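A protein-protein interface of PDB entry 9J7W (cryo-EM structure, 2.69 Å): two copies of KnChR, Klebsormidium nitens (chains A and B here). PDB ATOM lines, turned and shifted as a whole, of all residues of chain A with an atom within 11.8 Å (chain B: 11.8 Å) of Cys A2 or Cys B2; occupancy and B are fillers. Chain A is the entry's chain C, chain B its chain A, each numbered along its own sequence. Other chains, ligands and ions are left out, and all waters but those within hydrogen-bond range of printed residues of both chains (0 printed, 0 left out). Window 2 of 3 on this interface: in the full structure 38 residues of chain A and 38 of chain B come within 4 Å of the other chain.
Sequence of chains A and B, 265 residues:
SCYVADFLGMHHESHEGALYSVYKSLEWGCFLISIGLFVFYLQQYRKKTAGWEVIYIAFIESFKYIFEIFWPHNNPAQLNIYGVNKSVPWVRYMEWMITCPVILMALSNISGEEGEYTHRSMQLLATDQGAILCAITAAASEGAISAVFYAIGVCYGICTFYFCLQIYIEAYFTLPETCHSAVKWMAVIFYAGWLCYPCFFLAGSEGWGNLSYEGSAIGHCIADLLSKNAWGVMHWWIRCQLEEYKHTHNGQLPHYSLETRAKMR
Hydrophobic or aromatic side chains of chain B within 4 Å of the printed part of chain A: Tyr B3, Ala B5, Met B10 and Tyr B82.
Of the 9 printed residues of chain A, 6 touch a printed residue of chain B.
Of the printed residues of chain B, Cys A2 touches Ser B1 (3.8 Å) and Cys B2 (3.4 Å).
Cys B2 touches just these residues of chain A: Ser A1 (3.8 Å) and Cys A2 (3.4 Å).
Printed residues of chain B within 4 Å of Ser A1: Cys B2.
No residue of chain B comes within 4 Å of Val A4.
Ser B1 touches one residue of chain A.
No residue of chain A comes within 4 Å of Val B4.
Of the printed residues of chain B, Ala A5 touches Tyr B82.
Printed residues of chain A within 4 Å of Tyr B3: Tyr A3 (3.6 Å) and Tyr A82 (3.9 Å).
Of the printed residues of chain B, Tyr A82 touches Tyr B3, Ala B5 and Met B10.
Printed residues of chain A within 4 Å of Met B10: Tyr A82 (3.99 Å).
Printed residues of chain B within 4 Å of Tyr A3: Tyr B3 (3.6 Å) and Tyr B82 (3.9 Å).
Asp A6 touches none of the printed residues of chain B.
The nearest residue of chain B that does not touch Cys A2 is Tyr B3 (4.9 Å).
The nearest residue of chain A that does not touch Cys B2 is Tyr A3 (4.9 Å).
The side-chain sulfur (SG) of Cys B2 sits at hydrogen-bond distance from the side-chain sulfur (SG) of Cys A2, 3.4 Å away.
The side-chain hydroxyl of Tyr B3 lies within hydrogen-bond range of the backbone carbonyl oxygen of Tyr B82 (3.1 Å).
The side-chain amide oxygen of Asn B85 is in hydrogen-bond range of the side-chain hydroxyl of Tyr B3, at 2.5 Å.
O of Tyr B82 lies close to OD1 of Asn B85 (2.5 Å).
The backbone carbonyl oxygen (O) of Tyr A82 lies within hydrogen-bond range of the side-chain hydroxyl (OH) of Tyr A3 (3.1 Å).
The side-chain hydroxyl (OH) of Tyr A3 lies within hydrogen-bond range of the side-chain amide oxygen (OD1) of Asn A85, 2.5 Å away.
The side-chain amide oxygen (OD1) of Asn A85 lies close to the backbone carbonyl oxygen (O) of Tyr A82, 2.5 Å away.
Ser A1 touches Cys B2, and with the chains exchanged Cys A2 touches Ser B1.
Tyr B3 touches its own counterpart, Tyr A3.
Ala A5 touches Tyr B82, and with the chains exchanged Tyr A82 touches Ala B5.
Met A10 touches Tyr B82, and with the chains exchanged Tyr A82 touches Met B10.
9 positions are printed for both chains.
Of the 10 pairs that touch across the chains among the printed residues, 10 have their exchanged pair printed and touching as well.
Ser A1 touches Cys B2 (O to SG, 3.8 Å).
Cys A2 touches Ser B1 (SG to O, 3.8 Å).
CD2 of Tyr A3 touches CD2 of Tyr B3 (3.6 Å).
CE2 of Tyr A3 touches CE1 of Tyr B82, 3.9 Å away.
Ala A5 touches Tyr B82 (CB to CZ, 3.97 Å).
Met A10 touches Tyr B82 (CE to CE2, 3.99 Å).
CE2 of Tyr B3 touches CE1 of Tyr A82 (3.9 Å).
CB of Ala B5 touches CZ of Tyr A82, at 3.98 Å.
Tyr A82 touches Met B10 (CE2 to CE, 3.99 Å).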
ATOM      1  N   SER A   1      16.151  -3.804  12.471  1.00  0.00           N
ATOM      2  CA  SER A   1      17.580  -3.420  12.298  1.00  0.00           C
ATOM      3  C   SER A   1      17.960  -2.311  13.274  1.00  0.00           C
ATOM      4  O   SER A   1      18.451  -1.256  12.872  1.00  0.00           O
ATOM      5  CB  SER A   1      17.844  -2.972  10.859  1.00  0.00           C
ATOM      6  OG  SER A   1      17.056  -1.846  10.520  1.00  0.00           O
ATOM      7  N   CYS A   2      17.726  -2.557  14.559  1.00  0.00           N
ATOM      8  CA  CYS A   2      18.064  -1.604  15.602  1.00  0.00           C
ATOM      9  C   CYS A   2      19.528  -1.752  16.007  1.00  0.00           C
ATOM     10  O   CYS A   2      20.198  -2.733  15.676  1.00  0.00           O
ATOM     11  CB  CYS A   2      17.162  -1.799  16.821  1.00  0.00           C
ATOM     12  SG  CYS A   2      15.405  -1.507  16.506  1.00  0.00           S
ATOM     13  N   TYR A   3      20.022  -0.751  16.732  1.00  0.00           N
ATOM     14  CA  TYR A   3      21.392  -0.736  17.233  1.00  0.00           C
ATOM     15  C   TYR A   3      21.379  -0.218  18.663  1.00  0.00           C
ATOM     16  O   TYR A   3      21.193   0.982  18.889  1.00  0.00           O
ATOM     17  CB  TYR A   3      22.296   0.131  16.356  1.00  0.00           C
ATOM     18  CG  TYR A   3      23.645   0.422  16.974  1.00  0.00           C
ATOM     19  CD1 TYR A   3      24.705  -0.460  16.824  1.00  0.00           C
ATOM     20  CD2 TYR A   3      23.857   1.577  17.713  1.00  0.00           C
ATOM     21  CE1 TYR A   3      25.938  -0.197  17.389  1.00  0.00           C
ATOM     22  CE2 TYR A   3      25.085   1.847  18.283  1.00  0.00           C
ATOM     23  CZ  TYR A   3      26.121   0.956  18.118  1.00  0.00           C
ATOM     24  OH  TYR A   3      27.343   1.226  18.682  1.00  0.00           O
ATOM     25  N   VAL A   4      21.571  -1.116  19.621  1.00  0.00           N
ATOM     26  CA  VAL A   4      21.755  -0.720  21.008  1.00  0.00           C
ATOM     27  C   VAL A   4      23.238  -0.476  21.249  1.00  0.00           C
ATOM     28  O   VAL A   4      24.106  -1.144  20.685  1.00  0.00           O
ATOM     29  CB  VAL A   4      21.189  -1.767  21.988  1.00  0.00           C
ATOM     30  CG1 VAL A   4      19.690  -1.906  21.794  1.00  0.00           C
ATOM     31  CG2 VAL A   4      21.885  -3.109  21.813  1.00  0.00           C
ATOM     32  N   ALA A   5      23.531   0.502  22.104  1.00  0.00           N
ATOM     33  CA  ALA A   5      24.895   0.983  22.268  1.00  0.00           C
ATOM     34  C   ALA A   5      25.690   0.101  23.222  1.00  0.00           C
ATOM     35  O   ALA A   5      26.731  -0.448  22.848  1.00  0.00           O
ATOM     36  CB  ALA A   5      24.879   2.424  22.770  1.00  0.00           C
ATOM     37  N   ASP A   6      25.206  -0.037  24.454  1.00  0.00           N
ATOM     38  CA  ASP A   6      25.898  -0.817  25.472  1.00  0.00           C
ATOM     39  C   ASP A   6      27.314  -0.296  25.690  1.00  0.00           C
ATOM     40  O   ASP A   6      28.288  -1.041  25.547  1.00  0.00           O
ATOM     41  CB  ASP A   6      25.931  -2.298  25.086  1.00  0.00           C
ATOM     42  CG  ASP A   6      26.516  -3.172  26.179  1.00  0.00           C
ATOM     43  OD1 ASP A   6      25.822  -3.402  27.192  1.00  0.00           O
ATOM     44  OD2 ASP A   6      27.668  -3.628  26.025  1.00  0.00           O
ATOM     45  N   MET A  10      25.863   3.730  30.483  1.00  0.00           N
ATOM     46  CA  MET A  10      24.577   4.029  29.861  1.00  0.00           C
ATOM     47  C   MET A  10      23.462   3.245  30.542  1.00  0.00           C
ATOM     48  O   MET A  10      22.525   3.845  31.076  1.00  0.00           O
ATOM     49  CB  MET A  10      24.610   3.733  28.360  1.00  0.00           C
ATOM     50  CG  MET A  10      25.528   4.637  27.563  1.00  0.00           C
ATOM     51  SD  MET A  10      25.573   4.175  25.823  1.00  0.00           S
ATOM     52  CE  MET A  10      23.936   4.673  25.304  1.00  0.00           C
ATOM     53  N   TYR A  82      31.541   4.105  17.954  1.00  0.00           N
ATOM     54  CA  TYR A  82      30.330   3.411  17.524  1.00  0.00           C
ATOM     55  C   TYR A  82      30.634   2.053  16.907  1.00  0.00           C
ATOM     56  O   TYR A  82      30.211   1.015  17.427  1.00  0.00           O
ATOM     57  CB  TYR A  82      29.585   4.300  16.526  1.00  0.00           C
ATOM     58  CG  TYR A  82      28.606   3.578  15.633  1.00  0.00           C
ATOM     59  CD1 TYR A  82      27.341   3.242  16.081  1.00  0.00           C
ATOM     60  CD2 TYR A  82      28.947   3.244  14.332  1.00  0.00           C
ATOM     61  CE1 TYR A  82      26.446   2.588  15.261  1.00  0.00           C
ATOM     62  CE2 TYR A  82      28.063   2.591  13.509  1.00  0.00           C
ATOM     63  CZ  TYR A  82      26.813   2.264  13.976  1.00  0.00           C
ATOM     64  OH  TYR A  82      25.928   1.611  13.151  1.00  0.00           O
ATOM     65  N   ASN A  85      32.320  -0.056  19.195  1.00  0.00           N
ATOM     66  CA  ASN A  85      31.568  -0.241  20.430  1.00  0.00           C
ATOM     67  C   ASN A  85      32.490  -0.171  21.642  1.00  0.00           C
ATOM     68  O   ASN A  85      32.439  -1.010  22.542  1.00  0.00           O
ATOM     69  CB  ASN A  85      30.805  -1.566  20.410  1.00  0.00           C
ATOM     70  CG  ASN A  85      29.682  -1.577  19.399  1.00  0.00           C
ATOM     71  OD1 ASN A  85      29.097  -0.540  19.091  1.00  0.00           O
ATOM     72  ND2 ASN A  85      29.372  -2.756  18.875  1.00  0.00           N
ATOM     73  N   SER B   1      12.497   1.882  17.360  1.00  0.00           N
ATOM     74  CA  SER B   1      13.564   2.621  18.093  1.00  0.00           C
ATOM     75  C   SER B   1      14.937   2.300  17.510  1.00  0.00           C
ATOM     76  O   SER B   1      15.843   1.874  18.227  1.00  0.00           O
ATOM     77  CB  SER B   1      13.528   2.276  19.583  1.00  0.00           C
ATOM     78  OG  SER B   1      13.744   0.891  19.794  1.00  0.00           O
ATOM     79  N   CYS B   2      15.080   2.506  16.206  1.00  0.00           N
ATOM     80  CA  CYS B   2      16.340   2.271  15.519  1.00  0.00           C
ATOM     81  C   CYS B   2      17.252   3.488  15.649  1.00  0.00           C
ATOM     82  O   CYS B   2      16.829   4.579  16.035  1.00  0.00           O
ATOM     83  CB  CYS B   2      16.098   1.951  14.045  1.00  0.00           C
ATOM     84  SG  CYS B   2      15.147   0.442  13.752  1.00  0.00           S
ATOM     85  N   TYR B   3      18.526   3.281  15.320  1.00  0.00           N
ATOM     86  CA  TYR B   3      19.533   4.337  15.353  1.00  0.00           C
ATOM     87  C   TYR B   3      20.409   4.205  14.116  1.00  0.00           C
ATOM     88  O   TYR B   3      21.240   3.296  14.034  1.00  0.00           O
ATOM     89  CB  TYR B   3      20.381   4.256  16.622  1.00  0.00           C
ATOM     90  CG  TYR B   3      21.617   5.128  16.583  1.00  0.00           C
ATOM     91  CD1 TYR B   3      21.562   6.461  16.959  1.00  0.00           C
ATOM     92  CD2 TYR B   3      22.838   4.616  16.166  1.00  0.00           C
ATOM     93  CE1 TYR B   3      22.689   7.260  16.923  1.00  0.00           C
ATOM     94  CE2 TYR B   3      23.968   5.407  16.125  1.00  0.00           C
ATOM     95  CZ  TYR B   3      23.888   6.727  16.504  1.00  0.00           C
ATOM     96  OH  TYR B   3      25.013   7.514  16.467  1.00  0.00           O
ATOM     97  N   VAL B   4      20.223   5.107  13.159  1.00  0.00           N
ATOM     98  CA  VAL B   4      21.113   5.192  12.013  1.00  0.00           C
ATOM     99  C   VAL B   4      22.260   6.131  12.362  1.00  0.00           C
ATOM    100  O   VAL B   4      22.096   7.118  13.085  1.00  0.00           O
ATOM    101  CB  VAL B   4      20.375   5.653  10.740  1.00  0.00           C
ATOM    102  CG1 VAL B   4      19.310   4.641  10.358  1.00  0.00           C
ATOM    103  CG2 VAL B   4      19.764   7.035  10.935  1.00  0.00           C
ATOM    104  N   ALA B   5      23.443   5.817  11.838  1.00  0.00           N
ATOM    105  CA  ALA B   5      24.661   6.498  12.253  1.00  0.00           C
ATOM    106  C   ALA B   5      24.844   7.820  11.519  1.00  0.00           C
ATOM    107  O   ALA B   5      24.936   8.878  12.148  1.00  0.00           O
ATOM    108  CB  ALA B   5      25.867   5.592  12.017  1.00  0.00           C
ATOM    109  N   ASP B   6      24.897   7.765  10.189  1.00  0.00           N
ATOM    110  CA  ASP B   6      25.115   8.954   9.376  1.00  0.00           C
ATOM    111  C   ASP B   6      26.412   9.652   9.766  1.00  0.00           C
ATOM    112  O   ASP B   6      26.406  10.833  10.126  1.00  0.00           O
ATOM    113  CB  ASP B   6      23.933   9.917   9.504  1.00  0.00           C
ATOM    114  CG  ASP B   6      24.045  11.105   8.568  1.00  0.00           C
ATOM    115  OD1 ASP B   6      23.829  10.927   7.351  1.00  0.00           O
ATOM    116  OD2 ASP B   6      24.351  12.216   9.048  1.00  0.00           O
ATOM    117  N   MET B  10      30.153   6.656   5.486  1.00  0.00           N
ATOM    118  CA  MET B  10      29.377   5.431   5.647  1.00  0.00           C
ATOM    119  C   MET B  10      28.393   5.270   4.495  1.00  0.00           C
ATOM    120  O   MET B  10      28.456   4.278   3.764  1.00  0.00           O
ATOM    121  CB  MET B  10      28.647   5.412   6.990  1.00  0.00           C
ATOM    122  CG  MET B  10      29.558   5.331   8.199  1.00  0.00           C
ATOM    123  SD  MET B  10      28.631   5.395   9.740  1.00  0.00           S
ATOM    124  CE  MET B  10      27.826   3.800   9.712  1.00  0.00           C
ATOM    125  N   TYR B  82      29.324   8.460  19.103  1.00  0.00           N
ATOM    126  CA  TYR B  82      27.950   7.991  18.954  1.00  0.00           C
ATOM    127  C   TYR B  82      26.935   9.029  19.411  1.00  0.00           C
ATOM    128  O   TYR B  82      26.123   9.512  18.614  1.00  0.00           O
ATOM    129  CB  TYR B  82      27.785   6.695  19.748  1.00  0.00           C
ATOM    130  CG  TYR B  82      26.363   6.336  20.102  1.00  0.00           C
ATOM    131  CD1 TYR B  82      25.528   5.727  19.183  1.00  0.00           C
ATOM    132  CD2 TYR B  82      25.861   6.598  21.366  1.00  0.00           C
ATOM    133  CE1 TYR B  82      24.229   5.395  19.511  1.00  0.00           C
ATOM    134  CE2 TYR B  82      24.569   6.272  21.702  1.00  0.00           C
ATOM    135  CZ  TYR B  82      23.756   5.671  20.772  1.00  0.00           C
ATOM    136  OH  TYR B  82      22.464   5.345  21.108  1.00  0.00           O
ATOM    137  N   ASN B  85      27.246  12.037  17.571  1.00  0.00           N
ATOM    138  CA  ASN B  85      27.106  11.822  16.136  1.00  0.00           C
ATOM    139  C   ASN B  85      28.142  12.631  15.364  1.00  0.00           C
ATOM    140  O   ASN B  85      27.830  13.309  14.382  1.00  0.00           O
ATOM    141  CB  ASN B  85      25.692  12.168  15.668  1.00  0.00           C
ATOM    142  CG  ASN B  85      24.652  11.206  16.194  1.00  0.00           C
ATOM    143  OD1 ASN B  85      24.937  10.035  16.435  1.00  0.00           O
ATOM    144  ND2 ASN B  85      23.434  11.698  16.376  1.00  0.00           N
